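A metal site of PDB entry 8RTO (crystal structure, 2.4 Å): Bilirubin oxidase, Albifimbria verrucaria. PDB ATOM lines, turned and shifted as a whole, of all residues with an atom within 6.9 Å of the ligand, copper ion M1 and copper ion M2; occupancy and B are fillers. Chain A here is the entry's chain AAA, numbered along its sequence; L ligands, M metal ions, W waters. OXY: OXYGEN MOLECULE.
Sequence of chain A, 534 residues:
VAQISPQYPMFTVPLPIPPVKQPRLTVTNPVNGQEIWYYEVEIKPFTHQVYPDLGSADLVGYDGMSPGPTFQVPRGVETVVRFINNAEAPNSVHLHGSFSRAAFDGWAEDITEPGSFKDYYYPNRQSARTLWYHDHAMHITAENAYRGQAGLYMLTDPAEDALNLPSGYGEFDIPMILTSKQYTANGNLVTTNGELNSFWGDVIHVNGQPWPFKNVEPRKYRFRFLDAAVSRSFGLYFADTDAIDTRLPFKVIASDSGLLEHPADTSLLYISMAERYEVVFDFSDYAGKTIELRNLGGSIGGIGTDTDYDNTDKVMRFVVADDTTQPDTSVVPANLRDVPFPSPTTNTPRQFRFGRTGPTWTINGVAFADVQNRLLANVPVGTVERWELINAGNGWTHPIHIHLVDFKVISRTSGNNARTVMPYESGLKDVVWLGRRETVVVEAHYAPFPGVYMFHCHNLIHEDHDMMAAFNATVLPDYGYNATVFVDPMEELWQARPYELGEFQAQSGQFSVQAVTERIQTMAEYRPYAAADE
O of His 134 sits at hydrogen-bond distance from N of His 94 (2.8 Å). The backbone carbonyl oxygen of Met 454 lies within hydrogen-bond range of the backbone NH of His 403 (3.0 Å). O of His 456 sits at hydrogen-bond distance from N of His 401. A ring nitrogen (ND1) of His 403 sits at hydrogen-bond distance from the side-chain carboxylate of Asp 105 (2.6 Å). The backbone NH (N) of His 96 is in hydrogen-bond range of the backbone carbonyl oxygen (O) of Trp 132. NH2 of Arg 276 is in hydrogen-bond range of NE2 of His 96, at 3.1 Å. A ring nitrogen (NE2) of His 96 sits close to a ring nitrogen (ND1) of His 401 (3.4 Å). A ring nitrogen (ND1) of His 456 lies close to the side-chain carboxylate of Glu 463 (2.8 Å).
Water W1 bridges a ring nitrogen (ND1) of His 134 and the side-chain carboxylate (OE1) of Glu 463.
Merely in contact with copper ion M2: Trp 132 (3.6 Å) and His 94 (3.97 Å). The nearest printed residue that does not touch copper ion M2 is Ala 274 (4.3 Å).
Residues that only touch copper ion M1: His 401. Four residues have an atom within 4 Å of copper ion M1: His 136, His 401, His 403 and His 456. The nearest printed residue that does not touch copper ion M1 is Met 454 (4.1 Å).
NE2 of His 401 lies close to O1 of the ligand (3.4 Å). CD2 of His 94 touches O1 of the ligand (3.2 Å). Hydrophobic or aromatic side chains that line the ligand: His 94, His 96, His 134, His 136, His 401, His 403, His 456 and His 458. Within 4 Å of the ligand: His 94, His 96, His 134, His 136, His 401, His 403, His 456 and His 458. The nearest printed residue that does not touch the ligand is Glu 463 (4.4 Å).
A ring nitrogen (NE2) of His 403 is bound to copper ion M1, 2.0 Å away. NE2 of His 136 binds copper ion M1, at 2.0 Å. A ring nitrogen (NE2) of His 456 binds copper ion M1 (2.1 Å). O1 of the ligand binds copper ion M1 (2.3 Å). Copper ion M1 has four donor atoms within binding distance.
Copper ion M2 is bound by NE2 of His 134 (1.9 Å), ND1 of His 96 (2.1 Å), NE2 of His 458 (2.2 Å) and O1 of the ligand (2.6 Å).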
ATOM      1  N   HIS A  94      13.860 -20.414  -7.024  1.00  0.00           N
ATOM      2  CA  HIS A  94      14.769 -19.740  -6.075  1.00  0.00           C
ATOM      3  C   HIS A  94      16.082 -19.362  -6.776  1.00  0.00           C
ATOM      4  O   HIS A  94      16.756 -20.240  -7.258  1.00  0.00           O
ATOM      5  CB  HIS A  94      14.993 -20.639  -4.864  1.00  0.00           C
ATOM      6  CG  HIS A  94      16.017 -20.012  -3.978  1.00  0.00           C
ATOM      7  ND1 HIS A  94      15.924 -18.683  -3.576  1.00  0.00           N
ATOM      8  CD2 HIS A  94      17.194 -20.461  -3.514  1.00  0.00           C
ATOM      9  CE1 HIS A  94      16.978 -18.384  -2.842  1.00  0.00           C
ATOM     10  NE2 HIS A  94      17.761 -19.444  -2.805  1.00  0.00           N
ATOM     11  N   LEU A  95      16.394 -18.055  -6.860  1.00  0.00           N
ATOM     12  CA  LEU A  95      17.750 -17.553  -7.228  1.00  0.00           C
ATOM     13  C   LEU A  95      18.653 -17.616  -5.976  1.00  0.00           C
ATOM     14  O   LEU A  95      18.645 -16.662  -5.171  1.00  0.00           O
ATOM     15  CB  LEU A  95      17.704 -16.155  -7.838  1.00  0.00           C
ATOM     16  CG  LEU A  95      19.009 -15.684  -8.511  1.00  0.00           C
ATOM     17  CD1 LEU A  95      19.564 -16.668  -9.517  1.00  0.00           C
ATOM     18  CD2 LEU A  95      18.843 -14.341  -9.204  1.00  0.00           C
ATOM     19  N   HIS A  96      19.390 -18.720  -5.855  1.00  0.00           N
ATOM     20  CA  HIS A  96      20.307 -19.044  -4.730  1.00  0.00           C
ATOM     21  C   HIS A  96      21.556 -18.165  -4.909  1.00  0.00           C
ATOM     22  O   HIS A  96      22.236 -18.286  -5.961  1.00  0.00           O
ATOM     23  CB  HIS A  96      20.562 -20.575  -4.685  1.00  0.00           C
ATOM     24  CG  HIS A  96      21.327 -21.015  -3.472  1.00  0.00           C
ATOM     25  ND1 HIS A  96      21.082 -22.222  -2.847  1.00  0.00           N
ATOM     26  CD2 HIS A  96      22.318 -20.415  -2.768  1.00  0.00           C
ATOM     27  CE1 HIS A  96      21.869 -22.333  -1.798  1.00  0.00           C
ATOM     28  NE2 HIS A  96      22.655 -21.233  -1.721  1.00  0.00           N
ATOM     29  N   GLY A  97      21.778 -17.274  -3.941  1.00  0.00           N
ATOM     30  CA  GLY A  97      22.872 -16.305  -3.950  1.00  0.00           C
ATOM     31  C   GLY A  97      22.373 -14.893  -4.106  1.00  0.00           C
ATOM     32  O   GLY A  97      23.255 -13.960  -4.075  1.00  0.00           O
ATOM     33  N   ASP A 105      11.873 -14.792  -4.029  1.00  0.00           N
ATOM     34  CA  ASP A 105      13.022 -15.560  -3.483  1.00  0.00           C
ATOM     35  C   ASP A 105      12.729 -17.051  -3.598  1.00  0.00           C
ATOM     36  O   ASP A 105      13.612 -17.853  -3.254  1.00  0.00           O
ATOM     37  CB  ASP A 105      13.324 -15.187  -2.040  1.00  0.00           C
ATOM     38  CG  ASP A 105      14.621 -15.766  -1.524  1.00  0.00           C
ATOM     39  OD1 ASP A 105      15.668 -15.513  -2.169  1.00  0.00           O
ATOM     40  OD2 ASP A 105      14.569 -16.489  -0.501  1.00  0.00           O
ATOM     41  N   GLY A 106      11.550 -17.454  -4.038  1.00  0.00           N
ATOM     42  CA  GLY A 106      11.278 -18.902  -4.186  1.00  0.00           C
ATOM     43  C   GLY A 106      10.780 -19.550  -2.907  1.00  0.00           C
ATOM     44  O   GLY A 106      11.037 -20.775  -2.719  1.00  0.00           O
ATOM     45  N   TRP A 132      22.884 -19.755  -8.689  1.00  0.00           N
ATOM     46  CA  TRP A 132      22.153 -20.754  -9.476  1.00  0.00           C
ATOM     47  C   TRP A 132      20.681 -20.677  -9.126  1.00  0.00           C
ATOM     48  O   TRP A 132      20.329 -20.310  -7.971  1.00  0.00           O
ATOM     49  CB  TRP A 132      22.738 -22.144  -9.299  1.00  0.00           C
ATOM     50  CG  TRP A 132      22.666 -22.718  -7.911  1.00  0.00           C
ATOM     51  CD1 TRP A 132      23.148 -22.181  -6.757  1.00  0.00           C
ATOM     52  CD2 TRP A 132      22.144 -24.002  -7.568  1.00  0.00           C
ATOM     53  NE1 TRP A 132      22.919 -23.037  -5.719  1.00  0.00           N
ATOM     54  CE2 TRP A 132      22.329 -24.183  -6.190  1.00  0.00           C
ATOM     55  CE3 TRP A 132      21.549 -25.035  -8.302  1.00  0.00           C
ATOM     56  CZ2 TRP A 132      21.931 -25.333  -5.521  1.00  0.00           C
ATOM     57  CZ3 TRP A 132      21.180 -26.182  -7.647  1.00  0.00           C
ATOM     58  CH2 TRP A 132      21.361 -26.334  -6.267  1.00  0.00           C
ATOM     59  N   HIS A 134      16.923 -22.568  -9.188  1.00  0.00           N
ATOM     60  CA  HIS A 134      16.430 -23.956  -9.080  1.00  0.00           C
ATOM     61  C   HIS A 134      15.079 -23.999  -8.397  1.00  0.00           C
ATOM     62  O   HIS A 134      14.629 -23.010  -7.747  1.00  0.00           O
ATOM     63  CB  HIS A 134      17.500 -24.808  -8.356  1.00  0.00           C
ATOM     64  CG  HIS A 134      17.717 -24.445  -6.918  1.00  0.00           C
ATOM     65  ND1 HIS A 134      16.812 -24.797  -5.919  1.00  0.00           N
ATOM     66  CD2 HIS A 134      18.757 -23.859  -6.292  1.00  0.00           C
ATOM     67  CE1 HIS A 134      17.281 -24.398  -4.760  1.00  0.00           C
ATOM     68  NE2 HIS A 134      18.495 -23.825  -4.956  1.00  0.00           N
ATOM     69  N   ASP A 135      14.410 -25.138  -8.571  1.00  0.00           N
ATOM     70  CA  ASP A 135      13.043 -25.325  -8.054  1.00  0.00           C
ATOM     71  C   ASP A 135      13.106 -25.408  -6.538  1.00  0.00           C
ATOM     72  O   ASP A 135      14.106 -25.984  -6.052  1.00  0.00           O
ATOM     73  CB  ASP A 135      12.381 -26.581  -8.554  1.00  0.00           C
ATOM     74  CG  ASP A 135      10.909 -26.491  -8.188  1.00  0.00           C
ATOM     75  OD1 ASP A 135      10.224 -25.588  -8.760  1.00  0.00           O
ATOM     76  OD2 ASP A 135      10.501 -27.231  -7.267  1.00  0.00           O
ATOM     77  N   HIS A 136      12.094 -24.857  -5.856  1.00  0.00           N
ATOM     78  CA  HIS A 136      12.010 -24.788  -4.370  1.00  0.00           C
ATOM     79  C   HIS A 136      10.577 -25.092  -3.877  1.00  0.00           C
ATOM     80  O   HIS A 136      10.307 -24.813  -2.692  1.00  0.00           O
ATOM     81  CB  HIS A 136      12.489 -23.422  -3.867  1.00  0.00           C
ATOM     82  CG  HIS A 136      13.138 -23.480  -2.532  1.00  0.00           C
ATOM     83  ND1 HIS A 136      12.474 -23.968  -1.415  1.00  0.00           N
ATOM     84  CD2 HIS A 136      14.382 -23.172  -2.133  1.00  0.00           C
ATOM     85  CE1 HIS A 136      13.322 -23.963  -0.379  1.00  0.00           C
ATOM     86  NE2 HIS A 136      14.500 -23.499  -0.795  1.00  0.00           N
ATOM     87  N   THR A 141      10.646 -30.407  -4.302  1.00  0.00           N
ATOM     88  CA  THR A 141      12.002 -29.869  -4.622  1.00  0.00           C
ATOM     89  C   THR A 141      12.966 -30.994  -5.089  1.00  0.00           C
ATOM     90  O   THR A 141      13.509 -30.890  -6.215  1.00  0.00           O
ATOM     91  CB  THR A 141      12.509 -29.077  -3.400  1.00  0.00           C
ATOM     92  OG1 THR A 141      11.600 -28.000  -3.148  1.00  0.00           O
ATOM     93  CG2 THR A 141      13.910 -28.531  -3.561  1.00  0.00           C
ATOM     94  N   ALA A 274      24.789 -27.511  -2.947  1.00  0.00           N
ATOM     95  CA  ALA A 274      24.441 -26.095  -3.206  1.00  0.00           C
ATOM     96  C   ALA A 274      25.638 -25.183  -2.944  1.00  0.00           C
ATOM     97  O   ALA A 274      25.523 -23.922  -3.184  1.00  0.00           O
ATOM     98  CB  ALA A 274      23.238 -25.723  -2.387  1.00  0.00           C
ATOM     99  N   ARG A 276      29.011 -23.472  -4.031  1.00  0.00           N
ATOM    100  CA  ARG A 276      29.767 -22.968  -5.224  1.00  0.00           C
ATOM    101  C   ARG A 276      31.205 -22.630  -4.809  1.00  0.00           C
ATOM    102  O   ARG A 276      31.377 -21.731  -3.910  1.00  0.00           O
ATOM    103  CB  ARG A 276      29.110 -21.703  -5.823  1.00  0.00           C
ATOM    104  CG  ARG A 276      27.817 -21.973  -6.567  1.00  0.00           C
ATOM    105  CD  ARG A 276      26.595 -21.968  -5.655  1.00  0.00           C
ATOM    106  NE  ARG A 276      26.328 -20.614  -5.185  1.00  0.00           N
ATOM    107  CZ  ARG A 276      25.847 -20.285  -3.976  1.00  0.00           C
ATOM    108  NH1 ARG A 276      25.724 -18.998  -3.693  1.00  0.00           N
ATOM    109  NH2 ARG A 276      25.494 -21.198  -3.060  1.00  0.00           N
ATOM    110  N   HIS A 401      21.689 -24.088   4.375  1.00  0.00           N
ATOM    111  CA  HIS A 401      21.441 -22.857   3.602  1.00  0.00           C
ATOM    112  C   HIS A 401      20.567 -21.874   4.393  1.00  0.00           C
ATOM    113  O   HIS A 401      19.463 -22.260   4.774  1.00  0.00           O
ATOM    114  CB  HIS A 401      20.786 -23.251   2.274  1.00  0.00           C
ATOM    115  CG  HIS A 401      20.590 -22.087   1.389  1.00  0.00           C
ATOM    116  ND1 HIS A 401      21.472 -21.004   1.405  1.00  0.00           N
ATOM    117  CD2 HIS A 401      19.614 -21.806   0.512  1.00  0.00           C
ATOM    118  CE1 HIS A 401      21.043 -20.107   0.536  1.00  0.00           C
ATOM    119  NE2 HIS A 401      19.902 -20.595  -0.041  1.00  0.00           N
ATOM    120  N   ILE A 402      21.019 -20.629   4.547  1.00  0.00           N
ATOM    121  CA  ILE A 402      20.195 -19.471   5.003  1.00  0.00           C
ATOM    122  C   ILE A 402      19.936 -18.551   3.800  1.00  0.00           C
ATOM    123  O   ILE A 402      20.913 -18.028   3.200  1.00  0.00           O
ATOM    124  CB  ILE A 402      20.902 -18.724   6.159  1.00  0.00           C
ATOM    125  CG1 ILE A 402      21.421 -19.739   7.196  1.00  0.00           C
ATOM    126  CG2 ILE A 402      20.008 -17.692   6.812  1.00  0.00           C
ATOM    127  CD1 ILE A 402      22.262 -19.163   8.271  1.00  0.00           C
ATOM    128  N   HIS A 403      18.667 -18.322   3.442  1.00  0.00           N
ATOM    129  CA  HIS A 403      18.273 -17.355   2.392  1.00  0.00           C
ATOM    130  C   HIS A 403      18.637 -15.938   2.880  1.00  0.00           C
ATOM    131  O   HIS A 403      18.914 -15.779   4.121  1.00  0.00           O
ATOM    132  CB  HIS A 403      16.789 -17.550   2.093  1.00  0.00           C
ATOM    133  CG  HIS A 403      16.448 -18.788   1.329  1.00  0.00           C
ATOM    134  ND1 HIS A 403      15.751 -18.749   0.134  1.00  0.00           N
ATOM    135  CD2 HIS A 403      16.729 -20.094   1.566  1.00  0.00           C
ATOM    136  CE1 HIS A 403      15.587 -19.981  -0.331  1.00  0.00           C
ATOM    137  NE2 HIS A 403      16.183 -20.841   0.536  1.00  0.00           N
ATOM    138  N   VAL A 431      25.837 -21.397   2.144  1.00  0.00           N
ATOM    139  CA  VAL A 431      25.731 -22.816   2.567  1.00  0.00           C
ATOM    140  C   VAL A 431      26.959 -23.174   3.417  1.00  0.00           C
ATOM    141  O   VAL A 431      28.094 -22.793   2.989  1.00  0.00           O
ATOM    142  CB  VAL A 431      25.613 -23.767   1.368  1.00  0.00           C
ATOM    143  CG1 VAL A 431      25.412 -25.205   1.806  1.00  0.00           C
ATOM    144  CG2 VAL A 431      24.500 -23.354   0.401  1.00  0.00           C
ATOM    145  N   MET A 454      13.466 -18.373   4.075  1.00  0.00           N
ATOM    146  CA  MET A 454      13.657 -19.794   4.426  1.00  0.00           C
ATOM    147  C   MET A 454      15.095 -20.036   4.884  1.00  0.00           C
ATOM    148  O   MET A 454      16.031 -19.308   4.517  1.00  0.00           O
ATOM    149  CB  MET A 454      13.356 -20.703   3.244  1.00  0.00           C
ATOM    150  CG  MET A 454      11.861 -20.883   3.022  1.00  0.00           C
ATOM    151  SD  MET A 454      11.440 -21.900   1.607  1.00  0.00           S
ATOM    152  CE  MET A 454      12.469 -21.092   0.371  1.00  0.00           C
ATOM    153  N   PHE A 455      15.254 -21.060   5.686  1.00  0.00           N
ATOM    154  CA  PHE A 455      16.554 -21.692   5.901  1.00  0.00           C
ATOM    155  C   PHE A 455      16.288 -23.162   6.111  1.00  0.00           C
ATOM    156  O   PHE A 455      15.183 -23.525   6.625  1.00  0.00           O
ATOM    157  CB  PHE A 455      17.333 -21.033   7.038  1.00  0.00           C
ATOM    158  CG  PHE A 455      16.930 -21.401   8.431  1.00  0.00           C
ATOM    159  CD1 PHE A 455      15.905 -20.717   9.073  1.00  0.00           C
ATOM    160  CD2 PHE A 455      17.658 -22.337   9.155  1.00  0.00           C
ATOM    161  CE1 PHE A 455      15.589 -20.974  10.393  1.00  0.00           C
ATOM    162  CE2 PHE A 455      17.342 -22.601  10.467  1.00  0.00           C
ATOM    163  CZ  PHE A 455      16.289 -21.932  11.083  1.00  0.00           C
ATOM    164  N   HIS A 456      17.289 -23.961   5.746  1.00  0.00           N
ATOM    165  CA  HIS A 456      17.096 -25.420   5.670  1.00  0.00           C
ATOM    166  C   HIS A 456      18.381 -26.142   5.310  1.00  0.00           C
ATOM    167  O   HIS A 456      19.368 -25.502   4.910  1.00  0.00           O
ATOM    168  CB  HIS A 456      16.079 -25.695   4.564  1.00  0.00           C
ATOM    169  CG  HIS A 456      16.497 -25.175   3.244  1.00  0.00           C
ATOM    170  ND1 HIS A 456      17.017 -25.980   2.264  1.00  0.00           N
ATOM    171  CD2 HIS A 456      16.410 -23.933   2.716  1.00  0.00           C
ATOM    172  CE1 HIS A 456      17.258 -25.248   1.196  1.00  0.00           C
ATOM    173  NE2 HIS A 456      16.855 -24.005   1.448  1.00  0.00           N
ATOM    174  N   CYS A 457      18.285 -27.460   5.353  1.00  0.00           N
ATOM    175  CA  CYS A 457      19.274 -28.381   4.805  1.00  0.00           C
ATOM    176  C   CYS A 457      19.068 -28.459   3.286  1.00  0.00           C
ATOM    177  O   CYS A 457      17.891 -28.431   2.881  1.00  0.00           O
ATOM    178  CB  CYS A 457      19.077 -29.724   5.485  1.00  0.00           C
ATOM    179  SG  CYS A 457      20.209 -30.959   4.825  1.00  0.00           S
ATOM    180  N   HIS A 458      20.150 -28.580   2.488  1.00  0.00           N
ATOM    181  CA  HIS A 458      20.110 -28.608   1.007  1.00  0.00           C
ATOM    182  C   HIS A 458      20.391 -30.018   0.467  1.00  0.00           C
ATOM    183  O   HIS A 458      20.467 -30.136  -0.781  1.00  0.00           O
ATOM    184  CB  HIS A 458      21.110 -27.612   0.383  1.00  0.00           C
ATOM    185  CG  HIS A 458      20.584 -26.886  -0.809  1.00  0.00           C
ATOM    186  ND1 HIS A 458      20.339 -27.511  -2.007  1.00  0.00           N
ATOM    187  CD2 HIS A 458      20.209 -25.597  -0.970  1.00  0.00           C
ATOM    188  CE1 HIS A 458      19.874 -26.623  -2.883  1.00  0.00           C
ATOM    189  NE2 HIS A 458      19.795 -25.438  -2.269  1.00  0.00           N
ATOM    190  N   LEU A 460      18.244 -32.522  -0.568  1.00  0.00           N
ATOM    191  CA  LEU A 460      16.879 -32.153  -0.998  1.00  0.00           C
ATOM    192  C   LEU A 460      15.894 -33.182  -0.437  1.00  0.00           C
ATOM    193  O   LEU A 460      14.759 -32.774  -0.175  1.00  0.00           O
ATOM    194  CB  LEU A 460      16.846 -32.068  -2.528  1.00  0.00           C
ATOM    195  CG  LEU A 460      17.824 -31.033  -3.093  1.00  0.00           C
ATOM    196  CD1 LEU A 460      17.683 -30.948  -4.611  1.00  0.00           C
ATOM    197  CD2 LEU A 460      17.602 -29.670  -2.440  1.00  0.00           C
ATOM    198  N   GLU A 463      15.289 -31.757   3.095  1.00  0.00           N
ATOM    199  CA  GLU A 463      14.524 -30.497   2.878  1.00  0.00           C
ATOM    200  C   GLU A 463      13.051 -30.856   2.707  1.00  0.00           C
ATOM    201  O   GLU A 463      12.223 -30.170   3.285  1.00  0.00           O
ATOM    202  CB  GLU A 463      15.061 -29.775   1.644  1.00  0.00           C
ATOM    203  CG  GLU A 463      14.446 -28.398   1.387  1.00  0.00           C
ATOM    204  CD  GLU A 463      15.061 -27.629   0.218  1.00  0.00           C
ATOM    205  OE1 GLU A 463      16.316 -27.637   0.091  1.00  0.00           O
ATOM    206  OE2 GLU A 463      14.287 -26.998  -0.550  1.00  0.00           O
ATOM    207  N   MET A 468      13.224 -27.839   7.023  1.00  0.00           N
ATOM    208  CA  MET A 468      13.188 -26.424   6.590  1.00  0.00           C
ATOM    209  C   MET A 468      12.447 -25.617   7.669  1.00  0.00           C
ATOM    210  O   MET A 468      11.646 -26.204   8.420  1.00  0.00           O
ATOM    211  CB  MET A 468      12.505 -26.376   5.224  1.00  0.00           C
ATOM    212  CG  MET A 468      12.602 -25.059   4.513  1.00  0.00           C
ATOM    213  SD  MET A 468      12.506 -25.286   2.681  1.00  0.00           S
ATOM    214  CE  MET A 468      10.754 -25.693   2.557  1.00  0.00           C
HETATM  215  O1  OXY L   1      17.943 -22.938  -1.565  1.00  0.00           O
HETATM  216  O2  OXY L   1      17.228 -23.827  -1.856  1.00  0.00           O
HETATM  217 CU    CU M   1      16.225 -22.706  -0.035  1.00  0.00          CU
HETATM  218 CU    CU M   2      19.594 -23.623  -3.428  1.00  0.00          CU
HETATM  219 CU    CU M   3      18.923 -20.123  -1.393  1.00  0.00          CU
HETATM  220  O   HOH W   1      16.701 -26.626  -3.110  1.00  0.00           O
